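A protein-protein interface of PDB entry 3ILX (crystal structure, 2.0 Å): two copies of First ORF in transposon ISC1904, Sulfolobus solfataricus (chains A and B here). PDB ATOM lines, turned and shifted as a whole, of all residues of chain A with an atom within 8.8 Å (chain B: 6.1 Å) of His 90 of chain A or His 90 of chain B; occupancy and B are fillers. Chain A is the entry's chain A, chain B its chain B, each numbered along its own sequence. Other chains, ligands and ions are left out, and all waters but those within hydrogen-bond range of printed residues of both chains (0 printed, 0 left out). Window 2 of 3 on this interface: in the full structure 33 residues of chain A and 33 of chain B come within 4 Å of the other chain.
Printed residues of chain B that touch a printed residue of chain A: Leu 60, Glu 85, Val 86, Ala 89 and His 90.
Hydrophobic or aromatic side chains of chain B that line the printed part of chain A: Leu 60, Val 86, Ala 89 and His 90.
Of the 24 printed residues of chain A, 7 touch a printed residue of chain B.
Hydrophobic or aromatic side chains of chain A within 4 Å of the printed part of chain B: Leu 56, Leu 60, Val 86, Ala 89 and His 90.
Along chain A the printed residues that touch a printed residue of chain B span positions 56 to 90.
A ring nitrogen (ND1) of His 90 of chain A lies close to the backbone carbonyl oxygen (O) of Ile 59 of chain A.
O of Leu 60 of chain A lies close to ND1 of His 90 of chain A (3.4 Å).
OD1 of Asn 62 of chain A is in hydrogen-bond range of ND1 of His 90 of chain A (2.8 Å).
The side-chain amino group of Lys 88 of chain A lies within salt-bridge range of the side-chain carboxylate of Glu 85 of chain A.
The side-chain amide oxygen (OD1) of Asn 62 of chain B lies within hydrogen-bond range of a ring nitrogen (ND1) of His 90 of chain B.
The side-chain carboxylate (OE1) of Glu 85 of chain B lies within salt-bridge range of the side-chain amino group (NZ) of Lys 88 of chain B, at 3.1 Å.
Of the printed residues of chain A, His 90 of chain B touches His 90.
No residue of chain A comes within 4 Å of Asn 91 of chain B.
Of the printed residues of chain A, Glu 85 of chain B touches Leu 56 (3.7 Å), Arg 57 (2.9 Å) and Leu 60 (3.6 Å).
Printed residues of chain A within 4 Å of Val 86 of chain B: Val 86.
Of the printed residues of chain B, Glu 85 of chain A touches Leu 60.
The nearest residue of chain A that does not touch His 90 of chain B is Leu 60 of chain A (4.1 Å).
The nearest printed residue of chain B that does not touch Leu 60 of chain A is Val 86 of chain B (4.02 Å).
Leu 60 of chain A touches Glu 85 of chain B, and with the chains exchanged Glu 85 of chain A touches Leu 60 of chain B.
Leu 60 of chain A touches Ala 89 of chain B, and with the chains exchanged Ala 89 of chain A touches Leu 60 of chain B.
Val 86 of chain B touches its own counterpart, Val 86 of chain A.
His 90 of chain B touches its own counterpart, His 90 of chain A.
Positions printed for both chains: 59, 60, 61, 62, 64, 85, 86, 87, 88, 89, 90, 91 and 92.
Of the 8 pairs that touch across the chains among the printed residues, 6 have their exchanged pair printed and touching as well.
NH2 of Arg 57 of chain A lies within salt-bridge range of OE2 of Glu 85 of chain B, at 2.9 Å.
NE2 of His 90 of chain A lies within hydrogen-bond range of NE2 of His 90 of chain B (2.9 Å).
Among the printed residues, pairs that only touch across the chains: Val 86 of chain A with Val 86 of chain B, Leu 60 of chain A with Glu 85 of chain B, Ala 89 of chain A with Leu 60 of chain B, Leu 56 of chain A with Glu 85 of chain B, Glu 85 of chain A with Leu 60 of chain B and Leu 60 of chain A with Ala 89 of chain B.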
ATOM      1  N   ALA A   3     -15.092   3.722 -23.211  1.00  0.00           N
ATOM      2  CA  ALA A   3     -16.510   4.093 -22.994  1.00  0.00           C
ATOM      3  C   ALA A   3     -16.635   5.556 -23.435  1.00  0.00           C
ATOM      4  O   ALA A   3     -15.765   6.379 -23.107  1.00  0.00           O
ATOM      5  CB  ALA A   3     -16.865   3.929 -21.542  1.00  0.00           C
ATOM      6  N   LEU A  56     -29.446   5.277 -28.349  1.00  0.00           N
ATOM      7  CA  LEU A  56     -30.073   4.247 -27.514  1.00  0.00           C
ATOM      8  C   LEU A  56     -29.407   2.875 -27.713  1.00  0.00           C
ATOM      9  O   LEU A  56     -29.181   2.131 -26.745  1.00  0.00           O
ATOM     10  CB  LEU A  56     -31.574   4.141 -27.845  1.00  0.00           C
ATOM     11  CG  LEU A  56     -32.403   3.027 -27.212  1.00  0.00           C
ATOM     12  CD1 LEU A  56     -32.296   3.156 -25.715  1.00  0.00           C
ATOM     13  CD2 LEU A  56     -33.876   3.151 -27.641  1.00  0.00           C
ATOM     14  N   ARG A  57     -29.133   2.523 -28.967  1.00  0.00           N
ATOM     15  CA  ARG A  57     -28.472   1.265 -29.268  1.00  0.00           C
ATOM     16  C   ARG A  57     -27.046   1.247 -28.734  1.00  0.00           C
ATOM     17  O   ARG A  57     -26.590   0.228 -28.234  1.00  0.00           O
ATOM     18  CB  ARG A  57     -28.510   0.972 -30.770  1.00  0.00           C
ATOM     19  CG  ARG A  57     -29.914   0.644 -31.219  1.00  0.00           C
ATOM     20  CD  ARG A  57     -30.122   0.810 -32.715  1.00  0.00           C
ATOM     21  NE  ARG A  57     -31.547   0.643 -33.000  1.00  0.00           N
ATOM     22  CZ  ARG A  57     -32.147   0.968 -34.139  1.00  0.00           C
ATOM     23  NH1 ARG A  57     -31.458   1.512 -35.134  1.00  0.00           N
ATOM     24  NH2 ARG A  57     -33.446   0.748 -34.279  1.00  0.00           N
ATOM     25  N   MET A  58     -26.353   2.380 -28.811  1.00  0.00           N
ATOM     26  CA  MET A  58     -25.006   2.426 -28.268  1.00  0.00           C
ATOM     27  C   MET A  58     -25.001   2.213 -26.749  1.00  0.00           C
ATOM     28  O   MET A  58     -24.137   1.518 -26.236  1.00  0.00           O
ATOM     29  CB  MET A  58     -24.318   3.748 -28.611  1.00  0.00           C
ATOM     30  CG  MET A  58     -23.859   3.838 -30.048  1.00  0.00           C
ATOM     31  SD  MET A  58     -23.065   5.605 -30.294  1.00  0.00           S
ATOM     32  CE  MET A  58     -21.283   5.203 -29.576  1.00  0.00           C
ATOM     33  N   ILE A  59     -25.938   2.852 -26.047  1.00  0.00           N
ATOM     34  CA  ILE A  59     -26.034   2.701 -24.586  1.00  0.00           C
ATOM     35  C   ILE A  59     -26.268   1.232 -24.250  1.00  0.00           C
ATOM     36  O   ILE A  59     -25.573   0.652 -23.413  1.00  0.00           O
ATOM     37  CB  ILE A  59     -27.177   3.558 -23.995  1.00  0.00           C
ATOM     38  CG1 ILE A  59     -26.866   5.045 -24.150  1.00  0.00           C
ATOM     39  CG2 ILE A  59     -27.435   3.216 -22.500  1.00  0.00           C
ATOM     40  CD1 ILE A  59     -28.089   5.975 -23.961  1.00  0.00           C
ATOM     41  N   LEU A  60     -27.251   0.643 -24.932  1.00  0.00           N
ATOM     42  CA  LEU A  60     -27.643  -0.747 -24.759  1.00  0.00           C
ATOM     43  C   LEU A  60     -26.526  -1.728 -25.108  1.00  0.00           C
ATOM     44  O   LEU A  60     -26.491  -2.843 -24.566  1.00  0.00           O
ATOM     45  CB  LEU A  60     -28.882  -1.058 -25.603  1.00  0.00           C
ATOM     46  CG  LEU A  60     -30.226  -0.502 -25.114  1.00  0.00           C
ATOM     47  CD1 LEU A  60     -31.300  -0.548 -26.239  1.00  0.00           C
ATOM     48  CD2 LEU A  60     -30.694  -1.238 -23.854  1.00  0.00           C
ATOM     49  N   ASN A  61     -25.631  -1.313 -26.008  1.00  0.00           N
ATOM     50  CA  ASN A  61     -24.452  -2.094 -26.366  1.00  0.00           C
ATOM     51  C   ASN A  61     -23.221  -1.763 -25.500  1.00  0.00           C
ATOM     52  O   ASN A  61     -22.104  -2.137 -25.837  1.00  0.00           O
ATOM     53  CB  ASN A  61     -24.125  -1.951 -27.851  1.00  0.00           C
ATOM     54  CG  ASN A  61     -23.196  -3.082 -28.367  1.00  0.00           C
ATOM     55  OD1 ASN A  61     -23.184  -4.202 -27.839  1.00  0.00           O
ATOM     56  ND2 ASN A  61     -22.411  -2.780 -29.386  1.00  0.00           N
ATOM     57  N   ASN A  62     -23.439  -1.058 -24.399  1.00  0.00           N
ATOM     58  CA  ASN A  62     -22.377  -0.737 -23.455  1.00  0.00           C
ATOM     59  C   ASN A  62     -21.252   0.087 -24.061  1.00  0.00           C
ATOM     60  O   ASN A  62     -20.103  -0.118 -23.724  1.00  0.00           O
ATOM     61  CB  ASN A  62     -21.795  -2.021 -22.824  1.00  0.00           C
ATOM     62  CG  ASN A  62     -22.847  -2.826 -22.087  1.00  0.00           C
ATOM     63  OD1 ASN A  62     -23.582  -2.280 -21.268  1.00  0.00           O
ATOM     64  ND2 ASN A  62     -22.954  -4.108 -22.407  1.00  0.00           N
ATOM     65  N   GLU A  63     -21.576   1.011 -24.952  1.00  0.00           N
ATOM     66  CA  GLU A  63     -20.543   1.836 -25.591  1.00  0.00           C
ATOM     67  C   GLU A  63     -20.381   3.210 -24.917  1.00  0.00           C
ATOM     68  O   GLU A  63     -19.484   3.973 -25.249  1.00  0.00           O
ATOM     69  CB  GLU A  63     -20.851   2.038 -27.073  1.00  0.00           C
ATOM     70  CG  GLU A  63     -20.758   0.777 -27.883  1.00  0.00           C
ATOM     71  CD  GLU A  63     -21.296   0.932 -29.291  1.00  0.00           C
ATOM     72  OE1 GLU A  63     -20.841   1.823 -30.036  1.00  0.00           O
ATOM     73  OE2 GLU A  63     -22.171   0.132 -29.666  1.00  0.00           O
ATOM     74  N   VAL A  64     -21.261   3.504 -23.969  1.00  0.00           N
ATOM     75  CA  VAL A  64     -21.473   4.883 -23.521  1.00  0.00           C
ATOM     76  C   VAL A  64     -21.250   5.019 -22.022  1.00  0.00           C
ATOM     77  O   VAL A  64     -21.815   4.276 -21.217  1.00  0.00           O
ATOM     78  CB  VAL A  64     -22.878   5.422 -23.912  1.00  0.00           C
ATOM     79  CG1 VAL A  64     -22.934   6.940 -23.784  1.00  0.00           C
ATOM     80  CG2 VAL A  64     -23.237   5.041 -25.353  1.00  0.00           C
ATOM     81  N   SER A  65     -20.411   5.978 -21.666  1.00  0.00           N
ATOM     82  CA  SER A  65     -20.179   6.297 -20.276  1.00  0.00           C
ATOM     83  C   SER A  65     -21.121   7.406 -19.827  1.00  0.00           C
ATOM     84  O   SER A  65     -21.628   7.398 -18.696  1.00  0.00           O
ATOM     85  CB  SER A  65     -18.738   6.753 -20.096  1.00  0.00           C
ATOM     86  OG  SER A  65     -18.574   7.427 -18.858  1.00  0.00           O
ATOM     87  N   ARG A  66     -21.350   8.372 -20.708  1.00  0.00           N
ATOM     88  CA  ARG A  66     -22.085   9.569 -20.317  1.00  0.00           C
ATOM     89  C   ARG A  66     -22.759  10.258 -21.526  1.00  0.00           C
ATOM     90  O   ARG A  66     -22.155  10.364 -22.597  1.00  0.00           O
ATOM     91  CB  ARG A  66     -21.101  10.515 -19.613  1.00  0.00           C
ATOM     92  CG  ARG A  66     -21.746  11.622 -18.891  1.00  0.00           C
ATOM     93  CD  ARG A  66     -20.704  12.408 -18.114  1.00  0.00           C
ATOM     94  NE  ARG A  66     -20.282  11.788 -16.861  1.00  0.00           N
ATOM     95  CZ  ARG A  66     -19.404  12.347 -16.024  1.00  0.00           C
ATOM     96  NH1 ARG A  66     -18.854  13.523 -16.321  1.00  0.00           N
ATOM     97  NH2 ARG A  66     -19.062  11.740 -14.895  1.00  0.00           N
ATOM     98  N   ILE A  82     -37.678   5.980 -18.241  1.00  0.00           N
ATOM     99  CA  ILE A  82     -37.271   4.696 -18.814  1.00  0.00           C
ATOM    100  C   ILE A  82     -35.809   4.817 -19.270  1.00  0.00           C
ATOM    101  O   ILE A  82     -34.989   3.962 -18.966  1.00  0.00           O
ATOM    102  CB  ILE A  82     -38.200   4.248 -19.988  1.00  0.00           C
ATOM    103  CG1 ILE A  82     -39.587   3.914 -19.446  1.00  0.00           C
ATOM    104  CG2 ILE A  82     -37.596   3.017 -20.759  1.00  0.00           C
ATOM    105  CD1 ILE A  82     -40.651   3.954 -20.543  1.00  0.00           C
ATOM    106  N   LEU A  83     -35.464   5.904 -19.952  1.00  0.00           N
ATOM    107  CA  LEU A  83     -34.070   6.045 -20.393  1.00  0.00           C
ATOM    108  C   LEU A  83     -33.078   5.997 -19.246  1.00  0.00           C
ATOM    109  O   LEU A  83     -31.991   5.437 -19.390  1.00  0.00           O
ATOM    110  CB  LEU A  83     -33.845   7.327 -21.202  1.00  0.00           C
ATOM    111  CG  LEU A  83     -34.661   7.393 -22.483  1.00  0.00           C
ATOM    112  CD1 LEU A  83     -34.406   8.757 -23.120  1.00  0.00           C
ATOM    113  CD2 LEU A  83     -34.274   6.261 -23.473  1.00  0.00           C
ATOM    114  N   GLU A  84     -33.437   6.618 -18.122  1.00  0.00           N
ATOM    115  CA  GLU A  84     -32.557   6.646 -16.967  1.00  0.00           C
ATOM    116  C   GLU A  84     -32.360   5.233 -16.384  1.00  0.00           C
ATOM    117  O   GLU A  84     -31.282   4.868 -15.913  1.00  0.00           O
ATOM    118  CB  GLU A  84     -33.159   7.535 -15.889  1.00  0.00           C
ATOM    119  CG  GLU A  84     -33.202   9.031 -16.201  1.00  0.00           C
ATOM    120  CD  GLU A  84     -33.751   9.824 -15.007  1.00  0.00           C
ATOM    121  OE1 GLU A  84     -34.926   9.610 -14.581  1.00  0.00           O
ATOM    122  OE2 GLU A  84     -32.997  10.644 -14.472  1.00  0.00           O
ATOM    123  N   GLU A  85     -33.424   4.439 -16.413  1.00  0.00           N
ATOM    124  CA  GLU A  85     -33.342   3.076 -15.922  1.00  0.00           C
ATOM    125  C   GLU A  85     -32.401   2.300 -16.830  1.00  0.00           C
ATOM    126  O   GLU A  85     -31.526   1.566 -16.351  1.00  0.00           O
ATOM    127  CB  GLU A  85     -34.728   2.436 -15.863  1.00  0.00           C
ATOM    128  CG  GLU A  85     -35.643   2.951 -14.752  1.00  0.00           C
ATOM    129  CD  GLU A  85     -35.162   2.575 -13.381  1.00  0.00           C
ATOM    130  OE1 GLU A  85     -34.510   1.522 -13.222  1.00  0.00           O
ATOM    131  OE2 GLU A  85     -35.457   3.323 -12.428  1.00  0.00           O
ATOM    132  N   VAL A  86     -32.561   2.512 -18.143  1.00  0.00           N
ATOM    133  CA  VAL A  86     -31.708   1.877 -19.141  1.00  0.00           C
ATOM    134  C   VAL A  86     -30.246   2.238 -18.920  1.00  0.00           C
ATOM    135  O   VAL A  86     -29.370   1.371 -18.891  1.00  0.00           O
ATOM    136  CB  VAL A  86     -32.149   2.273 -20.577  1.00  0.00           C
ATOM    137  CG1 VAL A  86     -31.156   1.715 -21.620  1.00  0.00           C
ATOM    138  CG2 VAL A  86     -33.560   1.720 -20.847  1.00  0.00           C
ATOM    139  N   CYS A  87     -29.987   3.531 -18.744  1.00  0.00           N
ATOM    140  CA  CYS A  87     -28.610   3.996 -18.531  1.00  0.00           C
ATOM    141  C   CYS A  87     -28.001   3.416 -17.264  1.00  0.00           C
ATOM    142  O   CYS A  87     -26.824   3.023 -17.251  1.00  0.00           O
ATOM    143  CB  CYS A  87     -28.589   5.516 -18.489  1.00  0.00           C
ATOM    144  SG  CYS A  87     -28.843   6.187 -20.118  1.00  0.00           S
ATOM    145  N   LYS A  88     -28.802   3.355 -16.201  1.00  0.00           N
ATOM    146  CA  LYS A  88     -28.330   2.847 -14.915  1.00  0.00           C
ATOM    147  C   LYS A  88     -27.857   1.397 -15.096  1.00  0.00           C
ATOM    148  O   LYS A  88     -26.762   1.034 -14.681  1.00  0.00           O
ATOM    149  CB  LYS A  88     -29.415   2.993 -13.845  1.00  0.00           C
ATOM    150  CG  LYS A  88     -29.005   2.534 -12.433  1.00  0.00           C
ATOM    151  CD  LYS A  88     -30.042   2.967 -11.358  1.00  0.00           C
ATOM    152  CE  LYS A  88     -31.396   2.272 -11.552  1.00  0.00           C
ATOM    153  NZ  LYS A  88     -32.549   2.960 -10.858  1.00  0.00           N
ATOM    154  N   ALA A  89     -28.652   0.575 -15.764  1.00  0.00           N
ATOM    155  CA  ALA A  89     -28.266  -0.812 -16.011  1.00  0.00           C
ATOM    156  C   ALA A  89     -27.067  -0.940 -16.967  1.00  0.00           C
ATOM    157  O   ALA A  89     -26.429  -1.982 -17.008  1.00  0.00           O
ATOM    158  CB  ALA A  89     -29.471  -1.616 -16.553  1.00  0.00           C
ATOM    159  N   HIS A  90     -26.771   0.101 -17.739  1.00  0.00           N
ATOM    160  CA  HIS A  90     -25.670   0.013 -18.716  1.00  0.00           C
ATOM    161  C   HIS A  90     -24.497   0.947 -18.448  1.00  0.00           C
ATOM    162  O   HIS A  90     -23.801   1.373 -19.387  1.00  0.00           O
ATOM    163  CB  HIS A  90     -26.195   0.226 -20.128  1.00  0.00           C
ATOM    164  CG  HIS A  90     -26.944  -0.944 -20.650  1.00  0.00           C
ATOM    165  ND1 HIS A  90     -26.319  -2.001 -21.272  1.00  0.00           N
ATOM    166  CD2 HIS A  90     -28.261  -1.247 -20.616  1.00  0.00           C
ATOM    167  CE1 HIS A  90     -27.221  -2.901 -21.615  1.00  0.00           C
ATOM    168  NE2 HIS A  90     -28.410  -2.466 -21.230  1.00  0.00           N
ATOM    169  N   ASN A  91     -24.307   1.264 -17.165  1.00  0.00           N
ATOM    170  CA  ASN A  91     -23.139   1.984 -16.677  1.00  0.00           C
ATOM    171  C   ASN A  91     -22.987   3.332 -17.346  1.00  0.00           C
ATOM    172  O   ASN A  91     -21.885   3.824 -17.582  1.00  0.00           O
ATOM    173  CB  ASN A  91     -21.879   1.111 -16.808  1.00  0.00           C
ATOM    174  CG  ASN A  91     -22.005  -0.183 -16.036  1.00  0.00           C
ATOM    175  OD1 ASN A  91     -22.430  -0.180 -14.878  1.00  0.00           O
ATOM    176  ND2 ASN A  91     -21.677  -1.304 -16.681  1.00  0.00           N
ATOM    177  N   CYS A  92     -24.141   3.937 -17.583  1.00  0.00           N
ATOM    178  CA  CYS A  92     -24.242   5.176 -18.293  1.00  0.00           C
ATOM    179  C   CYS A  92     -25.038   6.170 -17.439  1.00  0.00           C
ATOM    180  O   CYS A  92     -25.995   5.804 -16.762  1.00  0.00           O
ATOM    181  CB  CYS A  92     -24.979   4.907 -19.620  1.00  0.00           C
ATOM    182  SG  CYS A  92     -24.927   6.291 -20.720  1.00  0.00           S
ATOM    183  N   GLU A  93     -24.647   7.429 -17.506  1.00  0.00           N
ATOM    184  CA  GLU A  93     -25.295   8.504 -16.768  1.00  0.00           C
ATOM    185  C   GLU A  93     -25.754   9.533 -17.787  1.00  0.00           C
ATOM    186  O   GLU A  93     -25.032   9.841 -18.710  1.00  0.00           O
ATOM    187  CB  GLU A  93     -24.261   9.085 -15.811  1.00  0.00           C
ATOM    188  CG  GLU A  93     -24.326  10.539 -15.520  1.00  0.00           C
ATOM    189  CD  GLU A  93     -23.121  10.981 -14.705  1.00  0.00           C
ATOM    190  OE1 GLU A  93     -21.969  10.515 -14.996  1.00  0.00           O
ATOM    191  OE2 GLU A  93     -23.325  11.785 -13.759  1.00  0.00           O
ATOM    192  N   ILE B  59     -35.780  -7.048 -17.032  1.00  0.00           N
ATOM    193  CA  ILE B  59     -35.431  -7.231 -18.458  1.00  0.00           C
ATOM    194  C   ILE B  59     -33.998  -6.781 -18.650  1.00  0.00           C
ATOM    195  O   ILE B  59     -33.208  -7.482 -19.267  1.00  0.00           O
ATOM    196  CB  ILE B  59     -36.375  -6.479 -19.429  1.00  0.00           C
ATOM    197  CG1 ILE B  59     -37.780  -7.087 -19.361  1.00  0.00           C
ATOM    198  CG2 ILE B  59     -35.814  -6.491 -20.862  1.00  0.00           C
ATOM    199  CD1 ILE B  59     -38.874  -6.165 -19.955  1.00  0.00           C
ATOM    200  N   LEU B  60     -33.648  -5.651 -18.043  1.00  0.00           N
ATOM    201  CA  LEU B  60     -32.313  -5.098 -18.187  1.00  0.00           C
ATOM    202  C   LEU B  60     -31.230  -5.939 -17.495  1.00  0.00           C
ATOM    203  O   LEU B  60     -30.059  -5.840 -17.836  1.00  0.00           O
ATOM    204  CB  LEU B  60     -32.276  -3.669 -17.655  1.00  0.00           C
ATOM    205  CG  LEU B  60     -33.010  -2.611 -18.497  1.00  0.00           C
ATOM    206  CD1 LEU B  60     -33.381  -1.462 -17.572  1.00  0.00           C
ATOM    207  CD2 LEU B  60     -32.123  -2.146 -19.670  1.00  0.00           C
ATOM    208  N   ASN B  61     -31.646  -6.767 -16.545  1.00  0.00           N
ATOM    209  CA  ASN B  61     -30.735  -7.640 -15.831  1.00  0.00           C
ATOM    210  C   ASN B  61     -30.741  -9.030 -16.433  1.00  0.00           C
ATOM    211  O   ASN B  61     -30.301  -9.996 -15.788  1.00  0.00           O
ATOM    212  CB  ASN B  61     -31.108  -7.721 -14.349  1.00  0.00           C
ATOM    213  CG  ASN B  61     -29.990  -8.324 -13.507  1.00  0.00           C
ATOM    214  OD1 ASN B  61     -28.818  -8.032 -13.728  1.00  0.00           O
ATOM    215  ND2 ASN B  61     -30.344  -9.159 -12.538  1.00  0.00           N
ATOM    216  N   ASN B  62     -31.256  -9.130 -17.657  1.00  0.00           N
ATOM    217  CA  ASN B  62     -31.299 -10.389 -18.419  1.00  0.00           C
ATOM    218  C   ASN B  62     -31.988 -11.555 -17.736  1.00  0.00           C
ATOM    219  O   ASN B  62     -31.572 -12.723 -17.893  1.00  0.00           O
ATOM    220  CB  ASN B  62     -29.905 -10.819 -18.878  1.00  0.00           C
ATOM    221  CG  ASN B  62     -29.203  -9.742 -19.651  1.00  0.00           C
ATOM    222  OD1 ASN B  62     -29.627  -9.352 -20.743  1.00  0.00           O
ATOM    223  ND2 ASN B  62     -28.128  -9.239 -19.085  1.00  0.00           N
ATOM    224  N   VAL B  64     -35.262 -12.142 -18.243  1.00  0.00           N
ATOM    225  CA  VAL B  64     -36.552 -12.320 -18.914  1.00  0.00           C
ATOM    226  C   VAL B  64     -36.431 -12.776 -20.356  1.00  0.00           C
ATOM    227  O   VAL B  64     -35.720 -12.195 -21.154  1.00  0.00           O
ATOM    228  CB  VAL B  64     -37.410 -11.015 -18.882  1.00  0.00           C
ATOM    229  CG1 VAL B  64     -38.841 -11.284 -19.377  1.00  0.00           C
ATOM    230  CG2 VAL B  64     -37.466 -10.435 -17.502  1.00  0.00           C
ATOM    231  N   GLU B  85     -36.670  -1.756 -28.168  1.00  0.00           N
ATOM    232  CA  GLU B  85     -35.224  -1.747 -28.398  1.00  0.00           C
ATOM    233  C   GLU B  85     -34.525  -2.377 -27.194  1.00  0.00           C
ATOM    234  O   GLU B  85     -33.571  -3.126 -27.348  1.00  0.00           O
ATOM    235  CB  GLU B  85     -34.731  -0.315 -28.615  1.00  0.00           C
ATOM    236  CG  GLU B  85     -35.287   0.356 -29.868  1.00  0.00           C
ATOM    237  CD  GLU B  85     -34.642  -0.164 -31.142  1.00  0.00           C
ATOM    238  OE1 GLU B  85     -33.478  -0.654 -31.071  1.00  0.00           O
ATOM    239  OE2 GLU B  85     -35.299  -0.103 -32.216  1.00  0.00           O
ATOM    240  N   VAL B  86     -35.016  -2.050 -25.996  1.00  0.00           N
ATOM    241  CA  VAL B  86     -34.489  -2.600 -24.766  1.00  0.00           C
ATOM    242  C   VAL B  86     -34.593  -4.128 -24.745  1.00  0.00           C
ATOM    243  O   VAL B  86     -33.579  -4.810 -24.564  1.00  0.00           O
ATOM    244  CB  VAL B  86     -35.160  -1.953 -23.504  1.00  0.00           C
ATOM    245  CG1 VAL B  86     -34.735  -2.657 -22.225  1.00  0.00           C
ATOM    246  CG2 VAL B  86     -34.791  -0.462 -23.416  1.00  0.00           C
ATOM    247  N   CYS B  87     -35.800  -4.643 -24.981  1.00  0.00           N
ATOM    248  CA  CYS B  87     -36.054  -6.074 -24.962  1.00  0.00           C
ATOM    249  C   CYS B  87     -35.165  -6.813 -25.943  1.00  0.00           C
ATOM    250  O   CYS B  87     -34.543  -7.808 -25.562  1.00  0.00           O
ATOM    251  CB  CYS B  87     -37.503  -6.352 -25.296  1.00  0.00           C
ATOM    252  SG  CYS B  87     -38.539  -6.024 -23.893  1.00  0.00           S
ATOM    253  N   LYS B  88     -35.105  -6.317 -27.189  1.00  0.00           N
ATOM    254  CA  LYS B  88     -34.351  -6.951 -28.267  1.00  0.00           C
ATOM    255  C   LYS B  88     -32.883  -7.064 -27.864  1.00  0.00           C
ATOM    256  O   LYS B  88     -32.246  -8.088 -28.093  1.00  0.00           O
ATOM    257  CB  LYS B  88     -34.522  -6.171 -29.574  1.00  0.00           C
ATOM    258  CG  LYS B  88     -33.341  -6.247 -30.551  1.00  0.00           C
ATOM    259  CD  LYS B  88     -33.564  -5.465 -31.888  1.00  0.00           C
ATOM    260  CE  LYS B  88     -33.676  -3.933 -31.703  1.00  0.00           C
ATOM    261  NZ  LYS B  88     -33.496  -3.092 -32.956  1.00  0.00           N
ATOM    262  N   ALA B  89     -32.367  -6.015 -27.229  1.00  0.00           N
ATOM    263  CA  ALA B  89     -31.015  -6.005 -26.714  1.00  0.00           C
ATOM    264  C   ALA B  89     -30.768  -6.956 -25.554  1.00  0.00           C
ATOM    265  O   ALA B  89     -29.609  -7.259 -25.270  1.00  0.00           O
ATOM    266  CB  ALA B  89     -30.618  -4.581 -26.283  1.00  0.00           C
ATOM    267  N   HIS B  90     -31.823  -7.381 -24.855  1.00  0.00           N
ATOM    268  CA  HIS B  90     -31.655  -8.263 -23.717  1.00  0.00           C
ATOM    269  C   HIS B  90     -32.364  -9.557 -23.960  1.00  0.00           C
ATOM    270  O   HIS B  90     -32.795 -10.199 -23.003  1.00  0.00           O
ATOM    271  CB  HIS B  90     -32.184  -7.613 -22.432  1.00  0.00           C
ATOM    272  CG  HIS B  90     -31.327  -6.500 -21.943  1.00  0.00           C
ATOM    273  ND1 HIS B  90     -30.244  -6.707 -21.120  1.00  0.00           N
ATOM    274  CD2 HIS B  90     -31.371  -5.167 -22.186  1.00  0.00           C
ATOM    275  CE1 HIS B  90     -29.671  -5.548 -20.851  1.00  0.00           C
ATOM    276  NE2 HIS B  90     -30.338  -4.597 -21.484  1.00  0.00           N
ATOM    277  N   ASN B  91     -32.509  -9.903 -25.245  1.00  0.00           N
ATOM    278  CA  ASN B  91     -33.094 -11.171 -25.701  1.00  0.00           C
ATOM    279  C   ASN B  91     -34.437 -11.472 -25.092  1.00  0.00           C
ATOM    280  O   ASN B  91     -34.771 -12.621 -24.746  1.00  0.00           O
ATOM    281  CB  ASN B  91     -32.133 -12.311 -25.442  1.00  0.00           C
ATOM    282  CG  ASN B  91     -30.817 -12.066 -26.071  1.00  0.00           C
ATOM    283  OD1 ASN B  91     -30.743 -11.673 -27.244  1.00  0.00           O
ATOM    284  ND2 ASN B  91     -29.752 -12.247 -25.297  1.00  0.00           N
ATOM    285  N   CYS B  92     -35.212 -10.421 -24.968  1.00  0.00           N
ATOM    286  CA  CYS B  92     -36.501 -10.539 -24.396  1.00  0.00           C
ATOM    287  C   CYS B  92     -37.503 -10.234 -25.495  1.00  0.00           C
ATOM    288  O   CYS B  92     -37.287  -9.369 -26.316  1.00  0.00           O
ATOM    289  CB  CYS B  92     -36.632  -9.574 -23.230  1.00  0.00           C
ATOM    290  SG  CYS B  92     -38.206  -9.746 -22.416  1.00  0.00           S
